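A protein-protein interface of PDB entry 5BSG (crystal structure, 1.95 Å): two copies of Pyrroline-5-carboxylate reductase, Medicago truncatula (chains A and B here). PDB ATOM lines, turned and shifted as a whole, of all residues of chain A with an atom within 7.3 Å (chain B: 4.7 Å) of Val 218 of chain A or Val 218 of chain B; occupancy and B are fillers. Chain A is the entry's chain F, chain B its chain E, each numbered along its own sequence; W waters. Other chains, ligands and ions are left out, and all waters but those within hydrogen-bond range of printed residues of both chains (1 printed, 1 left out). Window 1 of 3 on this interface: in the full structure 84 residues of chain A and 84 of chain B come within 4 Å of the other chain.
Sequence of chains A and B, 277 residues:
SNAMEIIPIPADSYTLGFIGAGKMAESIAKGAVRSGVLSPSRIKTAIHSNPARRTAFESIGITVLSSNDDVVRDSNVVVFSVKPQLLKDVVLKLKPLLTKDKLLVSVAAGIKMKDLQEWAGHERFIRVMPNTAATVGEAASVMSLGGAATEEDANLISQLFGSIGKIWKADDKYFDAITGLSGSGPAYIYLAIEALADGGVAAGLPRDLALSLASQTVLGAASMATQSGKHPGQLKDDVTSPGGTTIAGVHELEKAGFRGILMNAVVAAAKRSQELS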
ATOM      1  N   ASN A 131     -27.762 -19.149 -27.180  1.00  0.00           N
ATOM      2  CA  ASN A 131     -26.671 -18.904 -26.251  1.00  0.00           C
ATOM      3  C   ASN A 131     -26.919 -19.628 -24.963  1.00  0.00           C
ATOM      4  O   ASN A 131     -27.939 -20.342 -24.830  1.00  0.00           O
ATOM      5  CB  ASN A 131     -26.389 -17.409 -26.104  1.00  0.00           C
ATOM      6  CG  ASN A 131     -27.376 -16.667 -25.231  1.00  0.00           C
ATOM      7  OD1 ASN A 131     -28.330 -17.211 -24.702  1.00  0.00           O
ATOM      8  ND2 ASN A 131     -27.200 -15.351 -25.161  1.00  0.00           N
ATOM      9  N   GLU A 138     -33.869 -17.849 -21.080  1.00  0.00           N
ATOM     10  CA  GLU A 138     -33.603 -16.467 -21.483  1.00  0.00           C
ATOM     11  C   GLU A 138     -32.478 -16.362 -22.554  1.00  0.00           C
ATOM     12  O   GLU A 138     -31.744 -15.377 -22.629  1.00  0.00           O
ATOM     13  CB  GLU A 138     -33.254 -15.653 -20.276  1.00  0.00           C
ATOM     14  CG  GLU A 138     -34.384 -15.417 -19.272  1.00  0.00           C
ATOM     15  CD  GLU A 138     -35.551 -14.596 -19.854  1.00  0.00           C
ATOM     16  OE1 GLU A 138     -35.450 -13.963 -20.970  1.00  0.00           O
ATOM     17  OE2 GLU A 138     -36.541 -14.508 -19.121  1.00  0.00           O
ATOM     18  N   ALA A 140     -30.732 -15.593 -26.003  1.00  0.00           N
ATOM     19  CA  ALA A 140     -30.833 -14.655 -27.149  1.00  0.00           C
ATOM     20  C   ALA A 140     -30.431 -15.519 -28.373  1.00  0.00           C
ATOM     21  O   ALA A 140     -29.262 -15.975 -28.475  1.00  0.00           O
ATOM     22  CB  ALA A 140     -29.869 -13.491 -26.983  1.00  0.00           C
ATOM     23  N   GLY A 185     -21.025 -12.781 -25.339  1.00  0.00           N
ATOM     24  CA  GLY A 185     -21.398 -11.761 -24.354  1.00  0.00           C
ATOM     25  C   GLY A 185     -21.720 -12.179 -22.941  1.00  0.00           C
ATOM     26  O   GLY A 185     -21.466 -11.435 -22.000  1.00  0.00           O
ATOM     27  N   PRO A 186     -22.309 -13.344 -22.759  1.00  0.00           N
ATOM     28  CA  PRO A 186     -22.634 -13.647 -21.371  1.00  0.00           C
ATOM     29  C   PRO A 186     -21.397 -13.677 -20.492  1.00  0.00           C
ATOM     30  O   PRO A 186     -21.461 -13.281 -19.337  1.00  0.00           O
ATOM     31  CB  PRO A 186     -23.268 -15.051 -21.439  1.00  0.00           C
ATOM     32  CG  PRO A 186     -23.927 -15.053 -22.804  1.00  0.00           C
ATOM     33  CD  PRO A 186     -22.935 -14.282 -23.702  1.00  0.00           C
ATOM     34  N   ILE A 189     -20.615 -10.289 -19.160  1.00  0.00           N
ATOM     35  CA  ILE A 189     -21.448  -9.926 -18.068  1.00  0.00           C
ATOM     36  C   ILE A 189     -21.126 -10.699 -16.776  1.00  0.00           C
ATOM     37  O   ILE A 189     -21.314 -10.166 -15.704  1.00  0.00           O
ATOM     38  CB  ILE A 189     -22.920 -10.074 -18.479  1.00  0.00           C
ATOM     39  CG1 ILE A 189     -23.173  -9.240 -19.751  1.00  0.00           C
ATOM     40  CG2 ILE A 189     -23.869  -9.666 -17.370  1.00  0.00           C
ATOM     41  CD1 ILE A 189     -22.718  -7.806 -19.674  1.00  0.00           C
ATOM     42  N   ALA A 192     -18.560  -8.790 -15.342  1.00  0.00           N
ATOM     43  CA  ALA A 192     -19.096  -7.559 -14.811  1.00  0.00           C
ATOM     44  C   ALA A 192     -19.777  -7.713 -13.460  1.00  0.00           C
ATOM     45  O   ALA A 192     -19.641  -6.928 -12.550  1.00  0.00           O
ATOM     46  CB  ALA A 192     -20.063  -6.937 -15.774  1.00  0.00           C
ATOM     47  N   ILE A 193     -20.506  -8.802 -13.334  1.00  0.00           N
ATOM     48  CA  ILE A 193     -21.150  -9.149 -12.075  1.00  0.00           C
ATOM     49  C   ILE A 193     -20.170  -9.358 -10.989  1.00  0.00           C
ATOM     50  O   ILE A 193     -20.354  -8.854  -9.846  1.00  0.00           O
ATOM     51  CB  ILE A 193     -22.140 -10.348 -12.234  1.00  0.00           C
ATOM     52  CG1 ILE A 193     -23.368  -9.887 -13.027  1.00  0.00           C
ATOM     53  CG2 ILE A 193     -22.600 -10.910 -10.886  1.00  0.00           C
ATOM     54  CD1 ILE A 193     -24.263 -11.052 -13.482  1.00  0.00           C
ATOM     55  N   LEU A 196     -18.582  -5.981 -10.068  1.00  0.00           N
ATOM     56  CA  LEU A 196     -19.514  -5.177  -9.297  1.00  0.00           C
ATOM     57  C   LEU A 196     -19.592  -5.625  -7.827  1.00  0.00           C
ATOM     58  O   LEU A 196     -19.564  -4.805  -6.907  1.00  0.00           O
ATOM     59  CB  LEU A 196     -20.922  -5.178  -9.879  1.00  0.00           C
ATOM     60  CG  LEU A 196     -21.057  -4.362 -11.192  1.00  0.00           C
ATOM     61  CD1 LEU A 196     -22.382  -4.694 -11.847  1.00  0.00           C
ATOM     62  CD2 LEU A 196     -20.989  -2.909 -10.936  1.00  0.00           C
ATOM     63  N   SER A 212     -25.421 -10.767  -4.356  1.00  0.00           N
ATOM     64  CA  SER A 212     -26.857 -10.740  -4.601  1.00  0.00           C
ATOM     65  C   SER A 212     -27.325  -9.454  -5.242  1.00  0.00           C
ATOM     66  O   SER A 212     -28.085  -9.462  -6.194  1.00  0.00           O
ATOM     67  CB  SER A 212     -27.664 -10.945  -3.286  1.00  0.00           C
ATOM     68  OG  SER A 212     -27.349 -12.203  -2.754  1.00  0.00           O
ATOM     69  N   LEU A 213     -26.798  -8.360  -4.761  1.00  0.00           N
ATOM     70  CA  LEU A 213     -27.164  -7.081  -5.334  1.00  0.00           C
ATOM     71  C   LEU A 213     -26.657  -6.937  -6.750  1.00  0.00           C
ATOM     72  O   LEU A 213     -27.363  -6.375  -7.614  1.00  0.00           O
ATOM     73  CB  LEU A 213     -26.669  -5.932  -4.457  1.00  0.00           C
ATOM     74  CG  LEU A 213     -27.383  -5.706  -3.124  1.00  0.00           C
ATOM     75  CD1 LEU A 213     -26.737  -4.575  -2.345  1.00  0.00           C
ATOM     76  CD2 LEU A 213     -28.886  -5.434  -3.276  1.00  0.00           C
ATOM     77  N   ALA A 214     -25.402  -7.346  -6.981  1.00  0.00           N
ATOM     78  CA  ALA A 214     -24.804  -7.173  -8.350  1.00  0.00           C
ATOM     79  C   ALA A 214     -25.646  -7.914  -9.368  1.00  0.00           C
ATOM     80  O   ALA A 214     -26.025  -7.351 -10.381  1.00  0.00           O
ATOM     81  CB  ALA A 214     -23.402  -7.718  -8.356  1.00  0.00           C
ATOM     82  N   SER A 215     -25.973  -9.172  -9.061  1.00  0.00           N
ATOM     83  CA  SER A 215     -26.742  -9.963 -10.017  1.00  0.00           C
ATOM     84  C   SER A 215     -28.103  -9.362 -10.269  1.00  0.00           C
ATOM     85  O   SER A 215     -28.536  -9.219 -11.430  1.00  0.00           O
ATOM     86  CB  SER A 215     -26.909 -11.439  -9.535  1.00  0.00           C
ATOM     87  OG  SER A 215     -25.629 -11.996  -9.468  1.00  0.00           O
ATOM     88  N   GLN A 216     -28.788  -8.984  -9.221  1.00  0.00           N
ATOM     89  CA  GLN A 216     -30.141  -8.489  -9.387  1.00  0.00           C
ATOM     90  C   GLN A 216     -30.173  -7.067  -9.993  1.00  0.00           C
ATOM     91  O   GLN A 216     -31.123  -6.694 -10.725  1.00  0.00           O
ATOM     92  CB  GLN A 216     -30.900  -8.488  -8.052  1.00  0.00           C
ATOM     93  CG  GLN A 216     -32.353  -7.957  -8.104  1.00  0.00           C
ATOM     94  CD  GLN A 216     -33.240  -8.887  -8.909  1.00  0.00           C
ATOM     95  OE1 GLN A 216     -33.006 -10.079  -9.009  1.00  0.00           O
ATOM     96  NE2 GLN A 216     -34.193  -8.302  -9.593  1.00  0.00           N
ATOM     97  N   THR A 217     -29.117  -6.311  -9.774  1.00  0.00           N
ATOM     98  CA  THR A 217     -29.032  -5.024 -10.410  1.00  0.00           C
ATOM     99  C   THR A 217     -28.881  -5.134 -11.944  1.00  0.00           C
ATOM    100  O   THR A 217     -29.522  -4.417 -12.688  1.00  0.00           O
ATOM    101  CB  THR A 217     -27.833  -4.212  -9.806  1.00  0.00           C
ATOM    102  OG1 THR A 217     -28.124  -3.968  -8.436  1.00  0.00           O
ATOM    103  CG2 THR A 217     -27.606  -2.868 -10.464  1.00  0.00           C
ATOM    104  N   VAL A 218     -28.034  -6.059 -12.372  1.00  0.00           N
ATOM    105  CA  VAL A 218     -27.850  -6.332 -13.793  1.00  0.00           C
ATOM    106  C   VAL A 218     -29.144  -6.829 -14.408  1.00  0.00           C
ATOM    107  O   VAL A 218     -29.561  -6.370 -15.431  1.00  0.00           O
ATOM    108  CB  VAL A 218     -26.684  -7.275 -14.045  1.00  0.00           C
ATOM    109  CG1 VAL A 218     -26.509  -7.515 -15.507  1.00  0.00           C
ATOM    110  CG2 VAL A 218     -25.370  -6.676 -13.513  1.00  0.00           C
ATOM    111  N   LEU A 219     -29.795  -7.752 -13.726  1.00  0.00           N
ATOM    112  CA  LEU A 219     -31.113  -8.292 -14.188  1.00  0.00           C
ATOM    113  C   LEU A 219     -32.126  -7.179 -14.371  1.00  0.00           C
ATOM    114  O   LEU A 219     -32.776  -7.063 -15.375  1.00  0.00           O
ATOM    115  CB  LEU A 219     -31.607  -9.375 -13.240  1.00  0.00           C
ATOM    116  CG  LEU A 219     -33.009  -9.977 -13.494  1.00  0.00           C
ATOM    117  CD1 LEU A 219     -32.998 -10.475 -14.842  1.00  0.00           C
ATOM    118  CD2 LEU A 219     -33.236 -11.192 -12.595  1.00  0.00           C
ATOM    119  N   GLY A 220     -32.251  -6.351 -13.351  1.00  0.00           N
ATOM    120  CA  GLY A 220     -33.221  -5.293 -13.381  1.00  0.00           C
ATOM    121  C   GLY A 220     -32.968  -4.280 -14.475  1.00  0.00           C
ATOM    122  O   GLY A 220     -33.875  -3.857 -15.176  1.00  0.00           O
ATOM    123  N   ALA A 221     -31.714  -3.859 -14.593  1.00  0.00           N
ATOM    124  CA  ALA A 221     -31.373  -2.900 -15.653  1.00  0.00           C
ATOM    125  C   ALA A 221     -31.681  -3.442 -17.040  1.00  0.00           C
ATOM    126  O   ALA A 221     -32.225  -2.765 -17.906  1.00  0.00           O
ATOM    127  CB  ALA A 221     -29.905  -2.487 -15.518  1.00  0.00           C
ATOM    128  N   ALA A 222     -31.342  -4.724 -17.244  1.00  0.00           N
ATOM    129  CA  ALA A 222     -31.593  -5.368 -18.519  1.00  0.00           C
ATOM    130  C   ALA A 222     -33.107  -5.515 -18.777  1.00  0.00           C
ATOM    131  O   ALA A 222     -33.556  -5.357 -19.914  1.00  0.00           O
ATOM    132  CB  ALA A 222     -30.912  -6.697 -18.619  1.00  0.00           C
ATOM    133  N   SER A 223     -33.861  -5.789 -17.737  1.00  0.00           N
ATOM    134  CA  SER A 223     -35.308  -5.839 -17.896  1.00  0.00           C
ATOM    135  C   SER A 223     -35.918  -4.485 -18.233  1.00  0.00           C
ATOM    136  O   SER A 223     -36.912  -4.395 -18.998  1.00  0.00           O
ATOM    137  CB  SER A 223     -35.960  -6.315 -16.607  1.00  0.00           C
ATOM    138  OG  SER A 223     -35.437  -7.556 -16.202  1.00  0.00           O
ATOM    139  N   MET A 224     -35.371  -3.409 -17.655  1.00  0.00           N
ATOM    140  CA  MET A 224     -35.801  -2.087 -18.027  1.00  0.00           C
ATOM    141  C   MET A 224     -35.513  -1.841 -19.500  1.00  0.00           C
ATOM    142  O   MET A 224     -36.296  -1.231 -20.244  1.00  0.00           O
ATOM    143  CB  MET A 224     -35.112  -0.995 -17.175  1.00  0.00           C
ATOM    144  CG  MET A 224     -35.536  -0.994 -15.716  1.00  0.00           C
ATOM    145  SD  MET A 224     -37.218  -0.368 -15.476  1.00  0.00           S
ATOM    146  CE  MET A 224     -36.979   1.382 -15.694  1.00  0.00           C
ATOM    147  N   ILE B 189     -24.895  -0.514 -16.286  1.00  0.00           N
ATOM    148  CA  ILE B 189     -25.390  -1.506 -17.220  1.00  0.00           C
ATOM    149  C   ILE B 189     -26.030  -0.892 -18.474  1.00  0.00           C
ATOM    150  O   ILE B 189     -25.930  -1.449 -19.526  1.00  0.00           O
ATOM    151  CB  ILE B 189     -26.347  -2.447 -16.475  1.00  0.00           C
ATOM    152  CG1 ILE B 189     -25.620  -3.058 -15.293  1.00  0.00           C
ATOM    153  CG2 ILE B 189     -26.861  -3.528 -17.430  1.00  0.00           C
ATOM    154  CD1 ILE B 189     -24.232  -3.694 -15.626  1.00  0.00           C
ATOM    155  N   ILE B 193     -24.889  -1.961 -22.153  1.00  0.00           N
ATOM    156  CA  ILE B 193     -25.788  -2.351 -23.191  1.00  0.00           C
ATOM    157  C   ILE B 193     -25.557  -1.563 -24.460  1.00  0.00           C
ATOM    158  O   ILE B 193     -25.495  -2.136 -25.554  1.00  0.00           O
ATOM    159  CB  ILE B 193     -27.266  -2.303 -22.728  1.00  0.00           C
ATOM    160  CG1 ILE B 193     -27.539  -3.460 -21.753  1.00  0.00           C
ATOM    161  CG2 ILE B 193     -28.213  -2.377 -23.888  1.00  0.00           C
ATOM    162  CD1 ILE B 193     -28.862  -3.351 -21.018  1.00  0.00           C
ATOM    163  N   LEU B 196     -22.157  -2.619 -25.942  1.00  0.00           N
ATOM    164  CA  LEU B 196     -22.292  -3.924 -26.607  1.00  0.00           C
ATOM    165  C   LEU B 196     -22.989  -3.840 -27.958  1.00  0.00           C
ATOM    166  O   LEU B 196     -22.518  -4.423 -28.941  1.00  0.00           O
ATOM    167  CB  LEU B 196     -23.057  -4.914 -25.726  1.00  0.00           C
ATOM    168  CG  LEU B 196     -22.256  -5.427 -24.538  1.00  0.00           C
ATOM    169  CD1 LEU B 196     -23.217  -6.176 -23.612  1.00  0.00           C
ATOM    170  CD2 LEU B 196     -21.171  -6.376 -24.939  1.00  0.00           C
ATOM    171  N   ALA B 214     -28.002  -7.243 -27.445  1.00  0.00           N
ATOM    172  CA  ALA B 214     -27.299  -6.733 -26.294  1.00  0.00           C
ATOM    173  C   ALA B 214     -28.165  -6.777 -25.039  1.00  0.00           C
ATOM    174  O   ALA B 214     -27.738  -7.356 -24.017  1.00  0.00           O
ATOM    175  CB  ALA B 214     -26.838  -5.325 -26.548  1.00  0.00           C
ATOM    176  N   SER B 215     -29.392  -6.278 -25.122  1.00  0.00           N
ATOM    177  CA  SER B 215     -30.243  -6.269 -23.970  1.00  0.00           C
ATOM    178  C   SER B 215     -30.579  -7.686 -23.489  1.00  0.00           C
ATOM    179  O   SER B 215     -30.515  -7.978 -22.305  1.00  0.00           O
ATOM    180  CB  SER B 215     -31.552  -5.520 -24.252  1.00  0.00           C
ATOM    181  OG  SER B 215     -31.232  -4.168 -24.532  1.00  0.00           O
ATOM    182  N   GLN B 216     -30.883  -8.551 -24.414  1.00  0.00           N
ATOM    183  CA  GLN B 216     -31.313  -9.905 -24.023  1.00  0.00           C
ATOM    184  C   GLN B 216     -30.118 -10.746 -23.558  1.00  0.00           C
ATOM    185  O   GLN B 216     -30.260 -11.642 -22.704  1.00  0.00           O
ATOM    186  CB  GLN B 216     -32.029 -10.650 -25.194  1.00  0.00           C
ATOM    187  CG  GLN B 216     -32.519 -12.040 -24.857  1.00  0.00           C
ATOM    188  CD  GLN B 216     -33.572 -12.029 -23.777  1.00  0.00           C
ATOM    189  OE1 GLN B 216     -34.358 -11.115 -23.663  1.00  0.00           O
ATOM    190  NE2 GLN B 216     -33.588 -13.055 -22.992  1.00  0.00           N
ATOM    191  N   THR B 217     -28.955 -10.458 -24.094  1.00  0.00           N
ATOM    192  CA  THR B 217     -27.701 -11.122 -23.606  1.00  0.00           C
ATOM    193  C   THR B 217     -27.395 -10.778 -22.135  1.00  0.00           C
ATOM    194  O   THR B 217     -27.150 -11.664 -21.310  1.00  0.00           O
ATOM    195  CB  THR B 217     -26.512 -10.784 -24.480  1.00  0.00           C
ATOM    196  OG1 THR B 217     -26.771 -11.297 -25.792  1.00  0.00           O
ATOM    197  CG2 THR B 217     -25.220 -11.397 -23.948  1.00  0.00           C
ATOM    198  N   VAL B 218     -27.572  -9.519 -21.803  1.00  0.00           N
ATOM    199  CA  VAL B 218     -27.401  -9.094 -20.454  1.00  0.00           C
ATOM    200  C   VAL B 218     -28.460  -9.713 -19.551  1.00  0.00           C
ATOM    201  O   VAL B 218     -28.135 -10.182 -18.461  1.00  0.00           O
ATOM    202  CB  VAL B 218     -27.332  -7.561 -20.345  1.00  0.00           C
ATOM    203  CG1 VAL B 218     -27.108  -7.124 -18.904  1.00  0.00           C
ATOM    204  CG2 VAL B 218     -26.182  -7.000 -21.181  1.00  0.00           C
ATOM    205  N   LEU B 219     -29.707  -9.687 -19.965  1.00  0.00           N
ATOM    206  CA  LEU B 219     -30.770 -10.244 -19.195  1.00  0.00           C
ATOM    207  C   LEU B 219     -30.519 -11.726 -18.920  1.00  0.00           C
ATOM    208  O   LEU B 219     -30.645 -12.211 -17.806  1.00  0.00           O
ATOM    209  CB  LEU B 219     -32.115 -10.024 -19.909  1.00  0.00           C
ATOM    210  CG  LEU B 219     -33.371 -10.686 -19.330  1.00  0.00           C
ATOM    211  CD1 LEU B 219     -33.486 -10.223 -17.964  1.00  0.00           C
ATOM    212  CD2 LEU B 219     -34.618 -10.215 -20.000  1.00  0.00           C
ATOM    213  N   GLY B 220     -30.142 -12.436 -19.965  1.00  0.00           N
ATOM    214  CA  GLY B 220     -29.901 -13.877 -19.847  1.00  0.00           C
ATOM    215  C   GLY B 220     -28.764 -14.235 -18.940  1.00  0.00           C
ATOM    216  O   GLY B 220     -28.886 -15.090 -18.092  1.00  0.00           O
ATOM    217  N   ALA B 221     -27.656 -13.548 -19.101  1.00  0.00           N
ATOM    218  CA  ALA B 221     -26.497 -13.769 -18.223  1.00  0.00           C
ATOM    219  C   ALA B 221     -26.803 -13.501 -16.749  1.00  0.00           C
ATOM    220  O   ALA B 221     -26.472 -14.295 -15.862  1.00  0.00           O
ATOM    221  CB  ALA B 221     -25.349 -12.924 -18.656  1.00  0.00           C
ATOM    222  N   ALA B 222     -27.548 -12.416 -16.497  1.00  0.00           N
ATOM    223  CA  ALA B 222     -27.949 -12.095 -15.129  1.00  0.00           C
ATOM    224  C   ALA B 222     -28.953 -13.115 -14.580  1.00  0.00           C
ATOM    225  O   ALA B 222     -28.853 -13.467 -13.387  1.00  0.00           O
ATOM    226  CB  ALA B 222     -28.566 -10.717 -15.025  1.00  0.00           C
HETATM  227  O   HOH W   1     -29.332 -14.168 -23.364  1.00  0.00           O
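The side-chain carboxylate of Glu 138 of chain A lies within hydrogen-bond range of the side-chain amide nitrogen of Gln 216 of chain B, 2.9 Å away.
The side-chain amide oxygen (OD1) of Asn 131 of chain A sits at hydrogen-bond distance from the backbone NH (N) of Ala 140 of chain A.
OG of Ser 223 of chain A is in hydrogen-bond range of O of Leu 219 of chain A (2.8 Å).
Among the printed residues, pairs that only touch across the chains: Glu 138 of chain A with Leu 219 of chain B (3.96 Å), Glu 138 of chain A with Gly 220 of chain B (3.7 Å), Ala 140 of chain A with Gln 216 of chain B (3.7 Å), Ala 140 of chain A with Thr 217 of chain B (3.98 Å), Gly 185 of chain A with Thr 217 of chain B (3.7 Å), Pro 186 of chain A with Thr 217 of chain B (3.7 Å), Pro 186 of chain A with Ala 221 of chain B (3.9 Å), Ile 189 of chain A with Val 218 of chain B (3.9 Å), Ile 189 of chain A with Ala 221 of chain B (3.7 Å), Ser 215 of chain A with Ala 222 of chain B (3.9 Å), Val 218 of chain A with Ile 189 of chain B (3.8 Å), Val 218 of chain A with Val 218 of chain B (3.5 Å), Val 218 of chain A with Ala 222 of chain B (3.8 Å), Leu 219 of chain A with Leu 219 of chain B (3.2 Å), Leu 219 of chain A with Ala 222 of chain B (3.5 Å), Ala 221 of chain A with Ile 189 of chain B (3.7 Å), Ala 222 of chain A with Ser 215 of chain B (3.9 Å), Ala 222 of chain A with Val 218 of chain B (3.8 Å), Ala 222 of chain A with Leu 219 of chain B (3.5 Å) and Ser 223 of chain A with Leu 219 of chain B (3.7 Å).
Val 218 of chain B touches just these residues of chain A: Ile 189, Val 218 and Ala 222.
Printed residues of chain A within 4 Å of Ile 189 of chain B: Val 218 and Ala 221.
Printed residues of chain B within 4 Å of Ser 215 of chain A: Ala 222 (3.9 Å).
Of the printed residues of chain A, Ala 222 of chain B touches Ser 215 (3.9 Å), Val 218 (3.8 Å) and Leu 219 (3.5 Å).
Printed residues of chain B within 4 Å of Ala 221 of chain A: Ile 189 (3.7 Å).
The nearest printed residue of chain B that does not touch Val 218 of chain A is Leu 219 of chain B (5.5 Å).
The nearest residue of chain A that does not touch Val 218 of chain B is Leu 219 of chain A (5.5 Å).
Printed residues of chain A that touch a printed residue of chain B: Glu 138, Ala 140, Gly 185, Pro 186, Ile 189, Ser 215, Val 218, Leu 219, Ala 221, Ala 222 and Ser 223.
Hydrophobic or aromatic side chains of chain A that line the printed part of chain B: Ala 140, Pro 186, Ile 189, Val 218, Leu 219, Ala 221 and Ala 222.
Of the 12 printed residues of chain B, 9 touch a printed residue of chain A.
Among the printed residues, 21 pairs touch across the chains.
Among the printed residues, no Asp or Glu carboxylate lies within 4 Å of a Lys or Arg side-chain nitrogen of the other chain.
Ser 215 of chain A touches Ala 222 of chain B, and with the chains exchanged Ala 222 of chain A touches Ser 215 of chain B.
Val 218 of chain A touches its own counterpart, Val 218 of chain B.
Leu 219 of chain A touches its own counterpart, Leu 219 of chain B.
Leu 219 of chain A touches Ala 222 of chain B, and with the chains exchanged Ala 222 of chain A touches Leu 219 of chain B.
Of the 21 pairs that touch across the chains among the printed residues, 12 have their exchanged pair printed and touching as well.
Water W1 lies within hydrogen-bond range of O of Gln 216 of chain B (2.8 Å), O of Glu 138 of chain A (2.8 Å), ND2 of Asn 131 of chain A (3.0 Å) and N of Ala 140 of chain A (3.3 Å).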
